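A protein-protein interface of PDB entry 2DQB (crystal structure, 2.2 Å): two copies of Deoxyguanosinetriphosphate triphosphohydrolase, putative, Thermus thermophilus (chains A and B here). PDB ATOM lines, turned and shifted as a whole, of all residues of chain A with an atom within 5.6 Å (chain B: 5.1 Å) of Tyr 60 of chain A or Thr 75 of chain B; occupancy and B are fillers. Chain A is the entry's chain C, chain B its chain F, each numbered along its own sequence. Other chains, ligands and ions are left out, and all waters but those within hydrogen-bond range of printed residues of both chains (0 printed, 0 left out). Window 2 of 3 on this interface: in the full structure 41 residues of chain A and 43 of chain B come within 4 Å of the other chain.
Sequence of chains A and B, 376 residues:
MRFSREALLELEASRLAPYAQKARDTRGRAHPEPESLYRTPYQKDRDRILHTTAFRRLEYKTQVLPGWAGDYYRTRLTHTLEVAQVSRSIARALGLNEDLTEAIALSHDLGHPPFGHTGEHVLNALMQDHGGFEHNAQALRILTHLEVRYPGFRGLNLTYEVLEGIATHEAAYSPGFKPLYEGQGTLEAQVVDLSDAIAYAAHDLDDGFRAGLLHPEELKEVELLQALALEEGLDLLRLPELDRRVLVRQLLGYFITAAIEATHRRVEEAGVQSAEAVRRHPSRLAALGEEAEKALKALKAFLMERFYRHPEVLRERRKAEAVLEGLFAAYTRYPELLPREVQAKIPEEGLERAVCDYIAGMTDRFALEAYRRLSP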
ATOM      1  N   ARG A  56       2.239  -7.978   9.713  1.00  0.00           N
ATOM      2  CA  ARG A  56       2.858  -6.938  10.525  1.00  0.00           C
ATOM      3  C   ARG A  56       3.388  -7.565  11.802  1.00  0.00           C
ATOM      4  O   ARG A  56       4.407  -7.138  12.317  1.00  0.00           O
ATOM      5  CB  ARG A  56       1.859  -5.841  10.897  1.00  0.00           C
ATOM      6  CG  ARG A  56       1.576  -4.860   9.780  1.00  0.00           C
ATOM      7  CD  ARG A  56       2.879  -4.234   9.249  1.00  0.00           C
ATOM      8  NE  ARG A  56       3.508  -3.345  10.225  1.00  0.00           N
ATOM      9  CZ  ARG A  56       3.084  -2.117  10.526  1.00  0.00           C
ATOM     10  NH1 ARG A  56       2.014  -1.592   9.928  1.00  0.00           N
ATOM     11  NH2 ARG A  56       3.741  -1.411  11.439  1.00  0.00           N
ATOM     12  N   ARG A  57       2.726  -8.611  12.291  1.00  0.00           N
ATOM     13  CA  ARG A  57       3.176  -9.191  13.544  1.00  0.00           C
ATOM     14  C   ARG A  57       4.406 -10.062  13.481  1.00  0.00           C
ATOM     15  O   ARG A  57       5.016 -10.337  14.509  1.00  0.00           O
ATOM     16  CB  ARG A  57       2.013  -9.877  14.258  1.00  0.00           C
ATOM     17  CG  ARG A  57       1.048  -8.840  14.779  1.00  0.00           C
ATOM     18  CD  ARG A  57      -0.170  -9.408  15.488  1.00  0.00           C
ATOM     19  NE  ARG A  57      -1.000  -8.324  16.029  1.00  0.00           N
ATOM     20  CZ  ARG A  57      -2.171  -8.491  16.638  1.00  0.00           C
ATOM     21  NH1 ARG A  57      -2.670  -9.709  16.800  1.00  0.00           N
ATOM     22  NH2 ARG A  57      -2.858  -7.433  17.064  1.00  0.00           N
ATOM     23  N   LEU A  58       4.794 -10.457  12.276  1.00  0.00           N
ATOM     24  CA  LEU A  58       5.998 -11.256  12.093  1.00  0.00           C
ATOM     25  C   LEU A  58       7.203 -10.422  12.549  1.00  0.00           C
ATOM     26  O   LEU A  58       8.255 -10.974  12.907  1.00  0.00           O
ATOM     27  CB  LEU A  58       6.200 -11.622  10.615  1.00  0.00           C
ATOM     28  CG  LEU A  58       5.119 -12.411   9.863  1.00  0.00           C
ATOM     29  CD1 LEU A  58       5.481 -12.478   8.353  1.00  0.00           C
ATOM     30  CD2 LEU A  58       5.028 -13.817  10.438  1.00  0.00           C
ATOM     31  N   GLU A  59       7.067  -9.095  12.507  1.00  0.00           N
ATOM     32  CA  GLU A  59       8.167  -8.224  12.919  1.00  0.00           C
ATOM     33  C   GLU A  59       8.313  -8.216  14.451  1.00  0.00           C
ATOM     34  O   GLU A  59       9.329  -7.769  14.976  1.00  0.00           O
ATOM     35  CB  GLU A  59       7.964  -6.793  12.394  1.00  0.00           C
ATOM     36  CG  GLU A  59       9.240  -5.945  12.502  1.00  0.00           C
ATOM     37  CD  GLU A  59       9.188  -4.616  11.763  1.00  0.00           C
ATOM     38  OE1 GLU A  59       8.150  -3.929  11.815  1.00  0.00           O
ATOM     39  OE2 GLU A  59      10.207  -4.244  11.149  1.00  0.00           O
ATOM     40  N   TYR A  60       7.303  -8.724  15.160  1.00  0.00           N
ATOM     41  CA  TYR A  60       7.356  -8.775  16.616  1.00  0.00           C
ATOM     42  C   TYR A  60       7.199 -10.175  17.171  1.00  0.00           C
ATOM     43  O   TYR A  60       6.668 -10.359  18.261  1.00  0.00           O
ATOM     44  CB  TYR A  60       6.296  -7.856  17.220  1.00  0.00           C
ATOM     45  CG  TYR A  60       6.414  -6.446  16.700  1.00  0.00           C
ATOM     46  CD1 TYR A  60       5.486  -5.941  15.786  1.00  0.00           C
ATOM     47  CD2 TYR A  60       7.490  -5.636  17.069  1.00  0.00           C
ATOM     48  CE1 TYR A  60       5.629  -4.667  15.247  1.00  0.00           C
ATOM     49  CE2 TYR A  60       7.639  -4.356  16.530  1.00  0.00           C
ATOM     50  CZ  TYR A  60       6.708  -3.884  15.622  1.00  0.00           C
ATOM     51  OH  TYR A  60       6.847  -2.630  15.076  1.00  0.00           O
ATOM     52  N   LYS A  61       7.655 -11.162  16.406  1.00  0.00           N
ATOM     53  CA  LYS A  61       7.603 -12.567  16.814  1.00  0.00           C
ATOM     54  C   LYS A  61       8.937 -13.132  16.369  1.00  0.00           C
ATOM     55  O   LYS A  61       9.295 -13.000  15.204  1.00  0.00           O
ATOM     56  CB  LYS A  61       6.459 -13.310  16.099  1.00  0.00           C
ATOM     57  CG  LYS A  61       5.050 -12.815  16.427  1.00  0.00           C
ATOM     58  CD  LYS A  61       3.969 -13.590  15.650  1.00  0.00           C
ATOM     59  CE  LYS A  61       3.266 -14.653  16.505  1.00  0.00           C
ATOM     60  NZ  LYS A  61       1.758 -14.477  16.608  1.00  0.00           N
ATOM     61  N   THR A  62       9.700 -13.737  17.268  1.00  0.00           N
ATOM     62  CA  THR A  62      10.979 -14.279  16.842  1.00  0.00           C
ATOM     63  C   THR A  62      10.857 -15.662  16.189  1.00  0.00           C
ATOM     64  O   THR A  62       9.859 -16.379  16.360  1.00  0.00           O
ATOM     65  CB  THR A  62      12.014 -14.324  18.016  1.00  0.00           C
ATOM     66  OG1 THR A  62      12.507 -12.998  18.291  1.00  0.00           O
ATOM     67  CG2 THR A  62      13.195 -15.157  17.645  1.00  0.00           C
ATOM     68  N   THR A  75      13.977 -12.306  13.585  1.00  0.00           N
ATOM     69  CA  THR A  75      12.546 -12.320  13.756  1.00  0.00           C
ATOM     70  C   THR A  75      11.919 -13.154  12.634  1.00  0.00           C
ATOM     71  O   THR A  75      12.624 -13.626  11.727  1.00  0.00           O
ATOM     72  CB  THR A  75      11.991 -10.913  13.701  1.00  0.00           C
ATOM     73  OG1 THR A  75      10.630 -10.947  14.128  1.00  0.00           O
ATOM     74  CG2 THR A  75      12.062 -10.357  12.280  1.00  0.00           C
ATOM     75  N   THR A 363       1.705 -11.004  19.589  1.00  0.00           N
ATOM     76  CA  THR A 363       3.132 -10.831  19.340  1.00  0.00           C
ATOM     77  C   THR A 363       3.764 -11.446  20.589  1.00  0.00           C
ATOM     78  O   THR A 363       3.056 -11.725  21.553  1.00  0.00           O
ATOM     79  CB  THR A 363       3.527  -9.342  19.256  1.00  0.00           C
ATOM     80  OG1 THR A 363       3.358  -8.727  20.545  1.00  0.00           O
ATOM     81  CG2 THR A 363       2.657  -8.617  18.217  1.00  0.00           C
ATOM     82  N   ASP A 364       5.075 -11.668  20.599  1.00  0.00           N
ATOM     83  CA  ASP A 364       5.700 -12.256  21.785  1.00  0.00           C
ATOM     84  C   ASP A 364       5.616 -11.348  23.013  1.00  0.00           C
ATOM     85  O   ASP A 364       5.250 -11.783  24.109  1.00  0.00           O
ATOM     86  CB  ASP A 364       7.168 -12.578  21.537  1.00  0.00           C
ATOM     87  CG  ASP A 364       7.387 -13.459  20.313  1.00  0.00           C
ATOM     88  OD1 ASP A 364       6.406 -13.988  19.754  1.00  0.00           O
ATOM     89  OD2 ASP A 364       8.553 -13.627  19.921  1.00  0.00           O
ATOM     90  N   ARG A 365       5.955 -10.082  22.837  1.00  0.00           N
ATOM     91  CA  ARG A 365       5.930  -9.166  23.962  1.00  0.00           C
ATOM     92  C   ARG A 365       4.531  -9.024  24.559  1.00  0.00           C
ATOM     93  O   ARG A 365       4.380  -9.098  25.774  1.00  0.00           O
ATOM     94  CB  ARG A 365       6.523  -7.801  23.554  1.00  0.00           C
ATOM     95  CG  ARG A 365       6.238  -6.604  24.497  1.00  0.00           C
ATOM     96  CD  ARG A 365       6.267  -6.923  26.009  1.00  0.00           C
ATOM     97  NE  ARG A 365       7.563  -7.375  26.520  1.00  0.00           N
ATOM     98  CZ  ARG A 365       8.708  -6.703  26.393  1.00  0.00           C
ATOM     99  NH1 ARG A 365       9.831  -7.206  26.907  1.00  0.00           N
ATOM    100  NH2 ARG A 365       8.741  -5.541  25.740  1.00  0.00           N
ATOM    101  N   LEU B  58      17.404  -1.846   9.999  1.00  0.00           N
ATOM    102  CA  LEU B  58      16.205  -1.098   9.643  1.00  0.00           C
ATOM    103  C   LEU B  58      15.081  -1.648  10.508  1.00  0.00           C
ATOM    104  O   LEU B  58      14.113  -0.963  10.792  1.00  0.00           O
ATOM    105  CB  LEU B  58      15.861  -1.311   8.160  1.00  0.00           C
ATOM    106  CG  LEU B  58      16.337  -0.305   7.114  1.00  0.00           C
ATOM    107  CD1 LEU B  58      17.737   0.181   7.452  1.00  0.00           C
ATOM    108  CD2 LEU B  58      16.291  -0.970   5.723  1.00  0.00           C
ATOM    109  N   GLU B  59      15.233  -2.896  10.930  1.00  0.00           N
ATOM    110  CA  GLU B  59      14.233  -3.556  11.757  1.00  0.00           C
ATOM    111  C   GLU B  59      14.216  -3.036  13.202  1.00  0.00           C
ATOM    112  O   GLU B  59      13.244  -3.235  13.929  1.00  0.00           O
ATOM    113  CB  GLU B  59      14.465  -5.074  11.741  1.00  0.00           C
ATOM    114  CG  GLU B  59      13.436  -5.852  12.519  1.00  0.00           C
ATOM    115  CD  GLU B  59      13.208  -7.265  11.984  1.00  0.00           C
ATOM    116  OE1 GLU B  59      14.192  -8.032  11.854  1.00  0.00           O
ATOM    117  OE2 GLU B  59      12.034  -7.605  11.700  1.00  0.00           O
ATOM    118  N   LYS B  61      15.135   0.308  13.905  1.00  0.00           N
ATOM    119  CA  LYS B  61      15.201   1.759  13.766  1.00  0.00           C
ATOM    120  C   LYS B  61      13.836   2.205  13.294  1.00  0.00           C
ATOM    121  O   LYS B  61      13.425   1.863  12.181  1.00  0.00           O
ATOM    122  CB  LYS B  61      16.249   2.158  12.740  1.00  0.00           C
ATOM    123  CG  LYS B  61      17.641   1.946  13.229  1.00  0.00           C
ATOM    124  CD  LYS B  61      18.669   1.996  12.107  1.00  0.00           C
ATOM    125  CE  LYS B  61      18.910   3.391  11.582  1.00  0.00           C
ATOM    126  NZ  LYS B  61      20.374   3.501  11.258  1.00  0.00           N
ATOM    127  N   THR B  62      13.119   2.957  14.125  1.00  0.00           N
ATOM    128  CA  THR B  62      11.791   3.396  13.734  1.00  0.00           C
ATOM    129  C   THR B  62      11.746   4.538  12.714  1.00  0.00           C
ATOM    130  O   THR B  62      12.731   5.239  12.472  1.00  0.00           O
ATOM    131  CB  THR B  62      10.943   3.766  14.978  1.00  0.00           C
ATOM    132  OG1 THR B  62      10.741   2.593  15.774  1.00  0.00           O
ATOM    133  CG2 THR B  62       9.571   4.298  14.568  1.00  0.00           C
ATOM    134  N   GLN B  63      10.579   4.664  12.096  1.00  0.00           N
ATOM    135  CA  GLN B  63      10.272   5.681  11.105  1.00  0.00           C
ATOM    136  C   GLN B  63       9.478   6.716  11.917  1.00  0.00           C
ATOM    137  O   GLN B  63       8.501   6.366  12.604  1.00  0.00           O
ATOM    138  CB  GLN B  63       9.381   5.074  10.009  1.00  0.00           C
ATOM    139  CG  GLN B  63       9.305   5.854   8.697  1.00  0.00           C
ATOM    140  CD  GLN B  63      10.420   5.477   7.746  1.00  0.00           C
ATOM    141  OE1 GLN B  63      10.882   4.335   7.740  1.00  0.00           O
ATOM    142  NE2 GLN B  63      10.852   6.430   6.925  1.00  0.00           N
ATOM    143  N   TYR B  73       4.100   2.699  15.881  1.00  0.00           N
ATOM    144  CA  TYR B  73       4.959   3.425  14.958  1.00  0.00           C
ATOM    145  C   TYR B  73       5.753   2.390  14.178  1.00  0.00           C
ATOM    146  O   TYR B  73       6.423   1.545  14.764  1.00  0.00           O
ATOM    147  CB  TYR B  73       5.885   4.361  15.732  1.00  0.00           C
ATOM    148  CG  TYR B  73       5.123   5.318  16.617  1.00  0.00           C
ATOM    149  CD1 TYR B  73       4.383   4.850  17.708  1.00  0.00           C
ATOM    150  CD2 TYR B  73       5.091   6.687  16.333  1.00  0.00           C
ATOM    151  CE1 TYR B  73       3.625   5.715  18.490  1.00  0.00           C
ATOM    152  CE2 TYR B  73       4.337   7.562  17.106  1.00  0.00           C
ATOM    153  CZ  TYR B  73       3.606   7.071  18.182  1.00  0.00           C
ATOM    154  OH  TYR B  73       2.846   7.931  18.943  1.00  0.00           O
ATOM    155  N   ARG B  74       5.665   2.448  12.855  1.00  0.00           N
ATOM    156  CA  ARG B  74       6.344   1.471  12.017  1.00  0.00           C
ATOM    157  C   ARG B  74       7.860   1.614  12.011  1.00  0.00           C
ATOM    158  O   ARG B  74       8.398   2.709  12.176  1.00  0.00           O
ATOM    159  CB  ARG B  74       5.790   1.542  10.588  1.00  0.00           C
ATOM    160  CG  ARG B  74       6.628   2.338   9.578  1.00  0.00           C
ATOM    161  CD  ARG B  74       5.822   2.592   8.290  1.00  0.00           C
ATOM    162  NE  ARG B  74       5.001   3.779   8.464  1.00  0.00           N
ATOM    163  CZ  ARG B  74       5.455   5.011   8.272  1.00  0.00           C
ATOM    164  NH1 ARG B  74       6.702   5.186   7.875  1.00  0.00           N
ATOM    165  NH2 ARG B  74       4.700   6.071   8.548  1.00  0.00           N
ATOM    166  N   THR B  75       8.541   0.487  11.842  1.00  0.00           N
ATOM    167  CA  THR B  75       9.990   0.464  11.796  1.00  0.00           C
ATOM    168  C   THR B  75      10.404   0.960  10.423  1.00  0.00           C
ATOM    169  O   THR B  75       9.564   1.119   9.524  1.00  0.00           O
ATOM    170  CB  THR B  75      10.549  -0.974  11.988  1.00  0.00           C
ATOM    171  OG1 THR B  75      10.251  -1.769  10.833  1.00  0.00           O
ATOM    172  CG2 THR B  75       9.898  -1.655  13.214  1.00  0.00           C
ATOM    173  N   ARG B  76      11.691   1.225  10.260  1.00  0.00           N
ATOM    174  CA  ARG B  76      12.182   1.643   8.972  1.00  0.00           C
ATOM    175  C   ARG B  76      12.157   0.445   8.008  1.00  0.00           C
ATOM    176  O   ARG B  76      12.136   0.651   6.801  1.00  0.00           O
ATOM    177  CB  ARG B  76      13.604   2.200   9.065  1.00  0.00           C
ATOM    178  CG  ARG B  76      13.695   3.686   9.393  1.00  0.00           C
ATOM    179  CD  ARG B  76      15.037   4.237   8.934  1.00  0.00           C
ATOM    180  NE  ARG B  76      15.226   5.657   9.239  1.00  0.00           N
ATOM    181  CZ  ARG B  76      14.358   6.628   8.952  1.00  0.00           C
ATOM    182  NH1 ARG B  76      13.212   6.355   8.350  1.00  0.00           N
ATOM    183  NH2 ARG B  76      14.650   7.887   9.253  1.00  0.00           N
ATOM    184  N   LEU B  77      12.156  -0.791   8.519  1.00  0.00           N
ATOM    185  CA  LEU B  77      12.123  -1.955   7.619  1.00  0.00           C
ATOM    186  C   LEU B  77      10.746  -2.039   6.967  1.00  0.00           C
ATOM    187  O   LEU B  77      10.639  -2.226   5.757  1.00  0.00           O
ATOM    188  CB  LEU B  77      12.438  -3.282   8.352  1.00  0.00           C
ATOM    189  CG  LEU B  77      12.271  -4.620   7.571  1.00  0.00           C
ATOM    190  CD1 LEU B  77      13.274  -4.702   6.431  1.00  0.00           C
ATOM    191  CD2 LEU B  77      12.460  -5.842   8.487  1.00  0.00           C
ATOM    192  N   THR B  78       9.695  -1.875   7.770  1.00  0.00           N
ATOM    193  CA  THR B  78       8.329  -1.931   7.274  1.00  0.00           C
ATOM    194  C   THR B  78       8.079  -0.856   6.225  1.00  0.00           C
ATOM    195  O   THR B  78       7.437  -1.116   5.204  1.00  0.00           O
ATOM    196  CB  THR B  78       7.314  -1.827   8.441  1.00  0.00           C
ATOM    197  OG1 THR B  78       7.228  -3.101   9.110  1.00  0.00           O
ATOM    198  CG2 THR B  78       5.932  -1.431   7.943  1.00  0.00           C
ATOM    199  N   HIS B  79       8.596   0.344   6.465  1.00  0.00           N
ATOM    200  CA  HIS B  79       8.457   1.444   5.517  1.00  0.00           C
ATOM    201  C   HIS B  79       9.119   1.083   4.175  1.00  0.00           C
ATOM    202  O   HIS B  79       8.568   1.331   3.099  1.00  0.00           O
ATOM    203  CB  HIS B  79       9.122   2.701   6.073  1.00  0.00           C
ATOM    204  CG  HIS B  79       9.237   3.818   5.085  1.00  0.00           C
ATOM    205  ND1 HIS B  79       8.156   4.566   4.675  1.00  0.00           N
ATOM    206  CD2 HIS B  79      10.311   4.318   4.425  1.00  0.00           C
ATOM    207  CE1 HIS B  79       8.554   5.475   3.803  1.00  0.00           C
ATOM    208  NE2 HIS B  79       9.858   5.344   3.635  1.00  0.00           N
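OE2 of Glu 59 of chain A sits at hydrogen-bond distance from OG1 of Thr 75 of chain B.
OE1 of Glu 59 of chain A sits at hydrogen-bond distance from OG1 of Thr 78 of chain B (3.0 Å).
Tyr 60 of chain A touches just one residue of chain B: Thr 75.
Of chain A, only Glu 59 and Tyr 60 come within 4 Å of Thr 75 of chain B.
Printed residues of chain A within 4 Å of Thr 78 of chain B: Arg 56 and Glu 59.
Printed residues of chain A within 4 Å of Arg 74 of chain B: Arg 56.
The nearest residue of chain A that does not touch Thr 75 of chain B is Arg 56 of chain A (5.2 Å).
Among the printed residues, merely in contact across the chains: Arg 56 of chain A with Arg 74 of chain B, Arg 56 of chain A with Thr 78 of chain B, Glu 59 of chain A with Glu 59 of chain B, Glu 59 of chain A with Leu 77 of chain B, Tyr 60 of chain A with Thr 75 of chain B and Thr 75 of chain A with Glu 59 of chain B.
Hydrophobic or aromatic side chains of chain B that line the printed part of chain A: Leu 77.
Hydrophobic or aromatic side chains of chain A within 4 Å of the printed part of chain B: Tyr 60.
Glu 59 of chain B touches its own counterpart, Glu 59 of chain A.
Glu 59 of chain A touches Thr 75 of chain B, and with the chains exchanged Thr 75 of chain A touches Glu 59 of chain B.
Positions printed for both chains: 58, 59, 61, 62 and 75.
Of the 8 pairs that touch across the chains among the printed residues, 3 have their exchanged pair printed and touching as well.
The backbone carbonyl oxygen (O) of Leu 58 of chain A is in hydrogen-bond range of the side-chain hydroxyl (OG1) of Thr 75 of chain A, 2.7 Å away.
The backbone carbonyl oxygen (O) of Lys 61 of chain A is in hydrogen-bond range of the side-chain hydroxyl (OG1) of Thr 75 of chain A, 2.7 Å away.
The backbone carbonyl oxygen (O) of Leu 58 of chain B lies within hydrogen-bond range of the backbone NH (N) of Leu 77 of chain B.
O of Arg 74 of chain B is in hydrogen-bond range of N of Gln 63 of chain B, at 2.9 Å.
OG1 of Thr 75 of chain B sits close to N of Leu 77 of chain B (3.2 Å).
The side-chain hydroxyl (OG1) of Thr 75 of chain B lies within hydrogen-bond range of the backbone NH (N) of Thr 78 of chain B, at 3.1 Å.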
